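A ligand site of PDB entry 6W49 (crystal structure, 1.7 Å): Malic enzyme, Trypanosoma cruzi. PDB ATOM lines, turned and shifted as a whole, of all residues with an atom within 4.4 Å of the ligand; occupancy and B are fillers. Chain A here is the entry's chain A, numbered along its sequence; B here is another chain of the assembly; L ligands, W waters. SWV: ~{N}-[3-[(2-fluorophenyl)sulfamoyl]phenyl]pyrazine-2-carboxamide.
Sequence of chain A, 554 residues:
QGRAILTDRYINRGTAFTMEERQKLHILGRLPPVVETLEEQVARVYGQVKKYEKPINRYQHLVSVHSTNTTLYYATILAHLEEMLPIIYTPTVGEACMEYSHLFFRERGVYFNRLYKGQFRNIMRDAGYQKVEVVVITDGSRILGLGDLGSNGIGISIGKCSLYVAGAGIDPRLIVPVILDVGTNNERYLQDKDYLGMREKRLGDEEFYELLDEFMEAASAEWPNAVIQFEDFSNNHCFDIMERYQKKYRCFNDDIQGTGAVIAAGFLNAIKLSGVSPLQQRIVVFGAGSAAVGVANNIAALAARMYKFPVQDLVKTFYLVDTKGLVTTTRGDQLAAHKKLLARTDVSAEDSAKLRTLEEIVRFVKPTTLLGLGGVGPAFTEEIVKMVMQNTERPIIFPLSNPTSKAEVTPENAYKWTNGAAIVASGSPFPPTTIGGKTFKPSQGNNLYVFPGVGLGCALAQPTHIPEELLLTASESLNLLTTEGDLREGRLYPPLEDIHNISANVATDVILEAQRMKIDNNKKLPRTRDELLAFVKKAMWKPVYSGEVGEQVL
OD1 of Asn 69 lies close to O of Asn 12, at 3.2 Å. The side-chain amide nitrogen of Asn 12 lies within hydrogen-bond range of the backbone carbonyl oxygen of Thr 68 (3.0 Å). The side-chain amide oxygen of Asn 12 lies within hydrogen-bond range of the backbone NH of Gly 14. The guanidinium group (NH1) of Arg 44 sits at hydrogen-bond distance from the side-chain amide oxygen (OE1) of Gln 48, at 3.2 Å. NH2 of Arg 44 sits at hydrogen-bond distance from OG1 of Thr 15, 3.4 Å away. The side-chain amide nitrogen of Gln 48 is in hydrogen-bond range of a ring nitrogen (NE2) of His 61 (2.9 Å). NE2 of Gln 41 sits at hydrogen-bond distance from OG1 of Thr 15. N of Leu 72 lies within hydrogen-bond range of OD1 of Asn 69.
Water W1 lies within hydrogen-bond range of the backbone carbonyl oxygen (O) of Arg 30, the backbone carbonyl oxygen (O) of Phe 105 of chain B and a nitrogen (N3) of the ligand. Water W2 bridges O of Arg 30 (2.7 Å) and O of Glu 107 of chain B (3.3 Å).
A nitrogen (N2) of the ligand sits close to the backbone carbonyl oxygen of Leu 6. NE2 of Gln 48 lies close to F1 of the ligand, at 3.0 Å. CG2 of Thr 7 touches N2 of the ligand, at 3.8 Å. Gly 14 touches the ligand (CA to O3, 3.6 Å). CD2 of Leu 31 touches N3 of the ligand, 3.6 Å away. Val 45 touches the ligand (CG2 to F1, 3.5 Å). CG2 of Val 65 touches C15 of the ligand, 3.7 Å away. CG2 of Thr 68 touches O1 of the ligand, at 3.4 Å. Leu 72 touches the ligand. CD of Arg 106 of chain B touches N2 of the ligand (3.5 Å). Glu 107 of chain B touches the ligand. Hydrophobic or aromatic side chains that line the ligand: Leu 6, Leu 31, Val 45, Val 65, Leu 72 and Phe 105 of chain B. Within 4 Å of the ligand: Leu 6, Thr 7, Asn 12, Gly 14, Thr 15, Leu 31, Gln 41, Arg 44, Val 45, Gln 48, Val 65, Thr 68, Asn 69, Leu 72, Phe 105 of chain B, Arg 106 of chain B and Glu 107 of chain B.
The side-chain amide nitrogen of Asn 12 is in hydrogen-bond range of an oxygen (O1) of the ligand (2.8 Å). An oxygen (O2) of the ligand sits at hydrogen-bond distance from the guanidinium group (NH2) of Arg 44, at 2.8 Å. The side-chain amide nitrogen of Gln 41 lies within hydrogen-bond range of an oxygen (O2) of the ligand (3.1 Å). O of Phe 105 of chain B is in hydrogen-bond range of N3 of the ligand (3.3 Å). The side-chain amide nitrogen (ND2) of Asn 69 sits at hydrogen-bond distance from an oxygen (O3) of the ligand. An oxygen (O2) of the ligand lies within hydrogen-bond range of the backbone NH (N) of Thr 15 (3.3 Å). The side-chain hydroxyl (OG1) of Thr 15 sits at hydrogen-bond distance from an oxygen (O2) of the ligand, at 3.3 Å.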
ATOM      1  N   LEU A   6       7.265  17.600 -17.529  1.00  0.00           N
ATOM      2  CA  LEU A   6       7.645  18.708 -16.609  1.00  0.00           C
ATOM      3  C   LEU A   6       8.593  18.173 -15.545  1.00  0.00           C
ATOM      4  O   LEU A   6       9.427  18.935 -15.085  1.00  0.00           O
ATOM      5  CB  LEU A   6       6.437  19.320 -15.908  1.00  0.00           C
ATOM      6  CG  LEU A   6       5.680  20.349 -16.736  1.00  0.00           C
ATOM      7  CD1 LEU A   6       4.380  20.700 -16.028  1.00  0.00           C
ATOM      8  CD2 LEU A   6       6.537  21.577 -16.990  1.00  0.00           C
ATOM      9  N   THR A   7       8.376  16.945 -15.062  1.00  0.00           N
ATOM     10  CA  THR A   7       9.067  16.423 -13.864  1.00  0.00           C
ATOM     11  C   THR A   7      10.315  15.637 -14.263  1.00  0.00           C
ATOM     12  O   THR A   7      10.946  15.110 -13.359  1.00  0.00           O
ATOM     13  CB  THR A   7       8.105  15.639 -12.950  1.00  0.00           C
ATOM     14  OG1 THR A   7       7.572  14.584 -13.740  1.00  0.00           O
ATOM     15  CG2 THR A   7       7.055  16.561 -12.372  1.00  0.00           C
ATOM     16  N   ASN A  12      12.283  18.466 -19.654  1.00  0.00           N
ATOM     17  CA  ASN A  12      11.510  19.664 -19.235  1.00  0.00           C
ATOM     18  C   ASN A  12      12.055  20.912 -19.948  1.00  0.00           C
ATOM     19  O   ASN A  12      13.237  21.160 -19.946  1.00  0.00           O
ATOM     20  CB  ASN A  12      11.579  19.872 -17.716  1.00  0.00           C
ATOM     21  CG  ASN A  12      10.762  21.054 -17.240  1.00  0.00           C
ATOM     22  OD1 ASN A  12       9.759  21.379 -17.871  1.00  0.00           O
ATOM     23  ND2 ASN A  12      11.218  21.708 -16.172  1.00  0.00           N
ATOM     24  N   GLY A  14      10.297  23.985 -19.104  1.00  0.00           N
ATOM     25  CA  GLY A  14       9.779  25.102 -18.302  1.00  0.00           C
ATOM     26  C   GLY A  14       8.996  26.083 -19.179  1.00  0.00           C
ATOM     27  O   GLY A  14       8.099  25.680 -19.985  1.00  0.00           O
ATOM     28  N   THR A  15       9.282  27.359 -19.022  1.00  0.00           N
ATOM     29  CA  THR A  15       8.524  28.428 -19.712  1.00  0.00           C
ATOM     30  C   THR A  15       8.765  28.434 -21.241  1.00  0.00           C
ATOM     31  O   THR A  15       8.114  29.230 -21.921  1.00  0.00           O
ATOM     32  CB  THR A  15       8.926  29.791 -19.143  1.00  0.00           C
ATOM     33  OG1 THR A  15      10.320  29.988 -19.384  1.00  0.00           O
ATOM     34  CG2 THR A  15       8.595  29.957 -17.677  1.00  0.00           C
ATOM     35  N   ARG A  30       0.162  24.627 -15.270  1.00  0.00           N
ATOM     36  CA  ARG A  30       1.307  24.184 -14.437  1.00  0.00           C
ATOM     37  C   ARG A  30       2.439  25.212 -14.412  1.00  0.00           C
ATOM     38  O   ARG A  30       3.479  25.001 -13.682  1.00  0.00           O
ATOM     39  CB  ARG A  30       1.896  22.888 -15.006  1.00  0.00           C
ATOM     40  CG  ARG A  30       0.903  21.739 -15.078  1.00  0.00           C
ATOM     41  CD  ARG A  30       1.349  20.701 -14.088  1.00  0.00           C
ATOM     42  NE  ARG A  30       0.626  19.455 -14.162  1.00  0.00           N
ATOM     43  CZ  ARG A  30       0.670  18.512 -13.221  1.00  0.00           C
ATOM     44  NH1 ARG A  30       1.425  18.709 -12.136  1.00  0.00           N
ATOM     45  NH2 ARG A  30      -0.024  17.397 -13.360  1.00  0.00           N
ATOM     46  N   LEU A  31       2.348  26.200 -15.287  1.00  0.00           N
ATOM     47  CA  LEU A  31       3.396  27.214 -15.546  1.00  0.00           C
ATOM     48  C   LEU A  31       2.771  28.598 -15.489  1.00  0.00           C
ATOM     49  O   LEU A  31       1.627  28.784 -15.895  1.00  0.00           O
ATOM     50  CB  LEU A  31       3.991  26.996 -16.943  1.00  0.00           C
ATOM     51  CG  LEU A  31       4.767  25.684 -17.121  1.00  0.00           C
ATOM     52  CD1 LEU A  31       5.007  25.457 -18.610  1.00  0.00           C
ATOM     53  CD2 LEU A  31       6.071  25.712 -16.376  1.00  0.00           C
ATOM     54  N   PRO A  32       3.569  29.627 -15.150  1.00  0.00           N
ATOM     55  CA  PRO A  32       3.141  31.011 -15.345  1.00  0.00           C
ATOM     56  C   PRO A  32       3.085  31.294 -16.852  1.00  0.00           C
ATOM     57  O   PRO A  32       3.627  30.504 -17.652  1.00  0.00           O
ATOM     58  CB  PRO A  32       4.211  31.808 -14.604  1.00  0.00           C
ATOM     59  CG  PRO A  32       5.467  30.976 -14.723  1.00  0.00           C
ATOM     60  CD  PRO A  32       4.980  29.537 -14.710  1.00  0.00           C
ATOM     61  N   GLN A  41      15.422  32.467 -21.342  1.00  0.00           N
ATOM     62  CA  GLN A  41      15.476  31.746 -20.048  1.00  0.00           C
ATOM     63  C   GLN A  41      16.914  31.871 -19.499  1.00  0.00           C
ATOM     64  O   GLN A  41      17.109  32.077 -18.294  1.00  0.00           O
ATOM     65  CB  GLN A  41      15.138  30.285 -20.245  1.00  0.00           C
ATOM     66  CG  GLN A  41      13.722  29.991 -20.655  1.00  0.00           C
ATOM     67  CD  GLN A  41      13.567  28.499 -20.829  1.00  0.00           C
ATOM     68  OE1 GLN A  41      14.269  27.846 -21.621  1.00  0.00           O
ATOM     69  NE2 GLN A  41      12.600  27.946 -20.116  1.00  0.00           N
ATOM     70  N   ARG A  44      17.481  35.163 -17.898  1.00  0.00           N
ATOM     71  CA  ARG A  44      16.731  35.231 -16.623  1.00  0.00           C
ATOM     72  C   ARG A  44      17.499  34.466 -15.562  1.00  0.00           C
ATOM     73  O   ARG A  44      17.774  35.052 -14.507  1.00  0.00           O
ATOM     74  CB  ARG A  44      15.319  34.686 -16.794  1.00  0.00           C
ATOM     75  CG  ARG A  44      14.600  34.493 -15.466  1.00  0.00           C
ATOM     76  CD  ARG A  44      13.144  34.256 -15.679  1.00  0.00           C
ATOM     77  NE  ARG A  44      12.883  33.116 -16.555  1.00  0.00           N
ATOM     78  CZ  ARG A  44      13.001  31.842 -16.245  1.00  0.00           C
ATOM     79  NH1 ARG A  44      13.394  31.464 -15.051  1.00  0.00           N
ATOM     80  NH2 ARG A  44      12.684  30.912 -17.123  1.00  0.00           N
ATOM     81  N   VAL A  45      17.944  33.260 -15.882  1.00  0.00           N
ATOM     82  CA  VAL A  45      18.741  32.460 -14.901  1.00  0.00           C
ATOM     83  C   VAL A  45      20.012  33.226 -14.535  1.00  0.00           C
ATOM     84  O   VAL A  45      20.363  33.250 -13.371  1.00  0.00           O
ATOM     85  CB  VAL A  45      19.077  31.064 -15.431  1.00  0.00           C
ATOM     86  CG1 VAL A  45      20.077  30.375 -14.504  1.00  0.00           C
ATOM     87  CG2 VAL A  45      17.832  30.198 -15.587  1.00  0.00           C
ATOM     88  N   GLN A  48      19.182  35.634 -11.971  1.00  0.00           N
ATOM     89  CA  GLN A  48      18.806  34.945 -10.714  1.00  0.00           C
ATOM     90  C   GLN A  48      20.116  34.568 -10.010  1.00  0.00           C
ATOM     91  O   GLN A  48      20.155  34.690  -8.770  1.00  0.00           O
ATOM     92  CB  GLN A  48      17.997  33.672 -10.987  1.00  0.00           C
ATOM     93  CG  GLN A  48      16.543  33.907 -11.458  1.00  0.00           C
ATOM     94  CD  GLN A  48      15.795  32.729 -12.035  1.00  0.00           C
ATOM     95  OE1 GLN A  48      14.668  32.905 -12.552  1.00  0.00           O
ATOM     96  NE2 GLN A  48      16.411  31.554 -11.999  1.00  0.00           N
ATOM     97  N   HIS A  61      21.914  27.919  -6.284  1.00  0.00           N
ATOM     98  CA  HIS A  61      20.912  28.309  -7.296  1.00  0.00           C
ATOM     99  C   HIS A  61      21.072  27.496  -8.585  1.00  0.00           C
ATOM    100  O   HIS A  61      20.085  26.952  -9.103  1.00  0.00           O
ATOM    101  CB  HIS A  61      20.946  29.779  -7.626  1.00  0.00           C
ATOM    102  CG  HIS A  61      19.827  30.103  -8.548  1.00  0.00           C
ATOM    103  ND1 HIS A  61      18.520  29.764  -8.201  1.00  0.00           N
ATOM    104  CD2 HIS A  61      19.784  30.525  -9.832  1.00  0.00           C
ATOM    105  CE1 HIS A  61      17.728  30.084  -9.216  1.00  0.00           C
ATOM    106  NE2 HIS A  61      18.482  30.568 -10.225  1.00  0.00           N
ATOM    107  N   SER A  64      19.686  24.060  -8.235  1.00  0.00           N
ATOM    108  CA  SER A  64      18.208  24.114  -8.353  1.00  0.00           C
ATOM    109  C   SER A  64      17.785  24.088  -9.837  1.00  0.00           C
ATOM    110  O   SER A  64      16.856  23.314 -10.225  1.00  0.00           O
ATOM    111  CB  SER A  64      17.692  25.298  -7.605  1.00  0.00           C
ATOM    112  OG  SER A  64      16.289  25.391  -7.759  1.00  0.00           O
ATOM    113  N   VAL A  65      18.424  24.892 -10.674  1.00  0.00           N
ATOM    114  CA  VAL A  65      18.149  24.871 -12.146  1.00  0.00           C
ATOM    115  C   VAL A  65      18.400  23.471 -12.709  1.00  0.00           C
ATOM    116  O   VAL A  65      17.526  22.943 -13.416  1.00  0.00           O
ATOM    117  CB  VAL A  65      18.980  25.928 -12.888  1.00  0.00           C
ATOM    118  CG1 VAL A  65      18.668  25.923 -14.380  1.00  0.00           C
ATOM    119  CG2 VAL A  65      18.770  27.298 -12.331  1.00  0.00           C
ATOM    120  N   THR A  68      15.814  20.749 -12.171  1.00  0.00           N
ATOM    121  CA  THR A  68      14.508  20.941 -12.817  1.00  0.00           C
ATOM    122  C   THR A  68      14.586  20.999 -14.343  1.00  0.00           C
ATOM    123  O   THR A  68      13.673  20.500 -14.998  1.00  0.00           O
ATOM    124  CB  THR A  68      13.852  22.180 -12.226  1.00  0.00           C
ATOM    125  OG1 THR A  68      13.588  21.855 -10.854  1.00  0.00           O
ATOM    126  CG2 THR A  68      12.600  22.548 -12.957  1.00  0.00           C
ATOM    127  N   ASN A  69      15.631  21.640 -14.860  1.00  0.00           N
ATOM    128  CA  ASN A  69      15.754  21.893 -16.311  1.00  0.00           C
ATOM    129  C   ASN A  69      17.207  21.746 -16.687  1.00  0.00           C
ATOM    130  O   ASN A  69      17.941  22.736 -16.644  1.00  0.00           O
ATOM    131  CB  ASN A  69      15.076  23.196 -16.663  1.00  0.00           C
ATOM    132  CG  ASN A  69      15.030  23.485 -18.142  1.00  0.00           C
ATOM    133  OD1 ASN A  69      15.742  22.864 -18.919  1.00  0.00           O
ATOM    134  ND2 ASN A  69      14.135  24.376 -18.575  1.00  0.00           N
ATOM    135  N   LEU A  72      18.450  23.926 -19.722  1.00  0.00           N
ATOM    136  CA  LEU A  72      18.621  25.338 -19.300  1.00  0.00           C
ATOM    137  C   LEU A  72      19.891  25.484 -18.469  1.00  0.00           C
ATOM    138  O   LEU A  72      20.604  26.479 -18.635  1.00  0.00           O
ATOM    139  CB  LEU A  72      17.387  25.797 -18.529  1.00  0.00           C
ATOM    140  CG  LEU A  72      17.439  27.184 -17.924  1.00  0.00           C
ATOM    141  CD1 LEU A  72      17.762  28.255 -18.975  1.00  0.00           C
ATOM    142  CD2 LEU A  72      16.068  27.475 -17.309  1.00  0.00           C
ATOM    143  N   HIS B 102      11.888  31.875  -7.925  1.00  0.00           N
ATOM    144  CA  HIS B 102      12.374  30.616  -8.497  1.00  0.00           C
ATOM    145  C   HIS B 102      12.343  29.479  -7.462  1.00  0.00           C
ATOM    146  O   HIS B 102      12.285  28.326  -7.861  1.00  0.00           O
ATOM    147  CB  HIS B 102      13.744  30.829  -9.123  1.00  0.00           C
ATOM    148  CG  HIS B 102      14.724  31.319  -8.109  1.00  0.00           C
ATOM    149  ND1 HIS B 102      15.331  30.483  -7.235  1.00  0.00           N
ATOM    150  CD2 HIS B 102      15.272  32.531  -7.922  1.00  0.00           C
ATOM    151  CE1 HIS B 102      16.162  31.171  -6.487  1.00  0.00           C
ATOM    152  NE2 HIS B 102      16.141  32.423  -6.859  1.00  0.00           N
ATOM    153  N   PHE B 105       9.303  27.194  -8.334  1.00  0.00           N
ATOM    154  CA  PHE B 105       9.008  26.758  -9.703  1.00  0.00           C
ATOM    155  C   PHE B 105       8.730  25.258  -9.768  1.00  0.00           C
ATOM    156  O   PHE B 105       7.775  24.844 -10.385  1.00  0.00           O
ATOM    157  CB  PHE B 105      10.172  27.153 -10.635  1.00  0.00           C
ATOM    158  CG  PHE B 105      10.362  28.610 -10.911  1.00  0.00           C
ATOM    159  CD1 PHE B 105       9.370  29.549 -10.677  1.00  0.00           C
ATOM    160  CD2 PHE B 105      11.509  29.030 -11.581  1.00  0.00           C
ATOM    161  CE1 PHE B 105       9.552  30.892 -11.018  1.00  0.00           C
ATOM    162  CE2 PHE B 105      11.675  30.344 -11.951  1.00  0.00           C
ATOM    163  CZ  PHE B 105      10.697  31.287 -11.676  1.00  0.00           C
ATOM    164  N   ARG B 106       9.519  24.453  -9.073  1.00  0.00           N
ATOM    165  CA  ARG B 106       9.430  22.975  -9.150  1.00  0.00           C
ATOM    166  C   ARG B 106       8.244  22.423  -8.339  1.00  0.00           C
ATOM    167  O   ARG B 106       7.761  21.275  -8.625  1.00  0.00           O
ATOM    168  CB  ARG B 106      10.729  22.335  -8.678  1.00  0.00           C
ATOM    169  CG  ARG B 106      10.731  20.816  -8.747  1.00  0.00           C
ATOM    170  CD  ARG B 106      10.375  20.189 -10.106  1.00  0.00           C
ATOM    171  NE  ARG B 106      10.369  18.724 -10.102  1.00  0.00           N
ATOM    172  CZ  ARG B 106       9.368  17.970  -9.642  1.00  0.00           C
ATOM    173  NH1 ARG B 106       9.467  16.648  -9.626  1.00  0.00           N
ATOM    174  NH2 ARG B 106       8.268  18.543  -9.174  1.00  0.00           N
ATOM    175  N   GLU B 107       7.644  23.215  -7.481  1.00  0.00           N
ATOM    176  CA  GLU B 107       6.500  22.783  -6.633  1.00  0.00           C
ATOM    177  C   GLU B 107       5.211  22.665  -7.428  1.00  0.00           C
ATOM    178  O   GLU B 107       5.078  23.202  -8.547  1.00  0.00           O
ATOM    179  CB  GLU B 107       6.232  23.752  -5.487  1.00  0.00           C
ATOM    180  CG  GLU B 107       7.446  23.984  -4.635  1.00  0.00           C
ATOM    181  CD  GLU B 107       8.037  22.740  -3.980  1.00  0.00           C
ATOM    182  OE1 GLU B 107       7.269  21.760  -3.593  1.00  0.00           O
ATOM    183  OE2 GLU B 107       9.247  22.771  -3.809  1.00  0.00           O
ATOM    184  N   LEU B 196       7.071  36.706 -14.837  1.00  0.00           N
ATOM    185  CA  LEU B 196       6.524  35.608 -15.681  1.00  0.00           C
ATOM    186  C   LEU B 196       4.996  35.618 -15.641  1.00  0.00           C
ATOM    187  O   LEU B 196       4.419  34.792 -16.287  1.00  0.00           O
ATOM    188  CB  LEU B 196       7.111  34.270 -15.207  1.00  0.00           C
ATOM    189  CG  LEU B 196       8.629  34.164 -15.341  1.00  0.00           C
ATOM    190  CD1 LEU B 196       9.121  32.813 -14.874  1.00  0.00           C
ATOM    191  CD2 LEU B 196       9.105  34.406 -16.788  1.00  0.00           C
HETATM  192  N1  SWV L   1       6.757  22.886 -12.591  1.00  0.00           N
HETATM  193  N3  SWV L   1       8.305  24.901 -13.645  1.00  0.00           N
HETATM  194  C4  SWV L   1       6.641  20.619 -11.901  1.00  0.00           C
HETATM  195  C5  SWV L   1       8.437  21.290 -13.072  1.00  0.00           C
HETATM  196  C6  SWV L   1       8.931  26.097 -14.065  1.00  0.00           C
HETATM  197  C7  SWV L   1       8.338  27.319 -13.716  1.00  0.00           C
HETATM  198  C8  SWV L   1       8.923  28.515 -14.095  1.00  0.00           C
HETATM  199  C10 SWV L   1      10.713  27.291 -15.123  1.00  0.00           C
HETATM  200  C13 SWV L   1      13.879  25.901 -12.137  1.00  0.00           C
HETATM  201  C15 SWV L   1      15.116  27.929 -11.942  1.00  0.00           C
HETATM  202  C17 SWV L   1      10.136  26.075 -14.782  1.00  0.00           C
HETATM  203  O1  SWV L   1       9.695  23.311 -14.503  1.00  0.00           O
HETATM  204  C1  SWV L   1       8.742  23.635 -13.821  1.00  0.00           C
HETATM  205  C2  SWV L   1       7.947  22.575 -13.112  1.00  0.00           C
HETATM  206  C3  SWV L   1       6.109  21.895 -11.993  1.00  0.00           C
HETATM  207  N2  SWV L   1       7.792  20.294 -12.453  1.00  0.00           N
HETATM  208  C9  SWV L   1      10.118  28.518 -14.795  1.00  0.00           C
HETATM  209  S1  SWV L   1      12.231  27.298 -16.038  1.00  0.00           S
HETATM  210  N4  SWV L   1      13.337  28.026 -15.151  1.00  0.00           N
HETATM  211  C11 SWV L   1      13.814  27.511 -13.918  1.00  0.00           C
HETATM  212  C12 SWV L   1      13.388  26.305 -13.370  1.00  0.00           C
HETATM  213  C14 SWV L   1      14.706  26.732 -11.408  1.00  0.00           C
HETATM  214  C16 SWV L   1      14.650  28.296 -13.167  1.00  0.00           C
HETATM  215  F1  SWV L   1      15.028  29.482 -13.649  1.00  0.00           F
HETATM  216  O2  SWV L   1      11.920  28.169 -17.150  1.00  0.00           O
HETATM  217  O3  SWV L   1      12.600  25.933 -16.275  1.00  0.00           O
HETATM  218  O   HOH W   1       5.483  26.211 -12.174  1.00  0.00           O
HETATM  219  O   HOH W   2       3.333  23.852 -11.253  1.00  0.00           O
HETATM  220  O   HOH W   3       4.605  19.690  -9.516  1.00  0.00           O
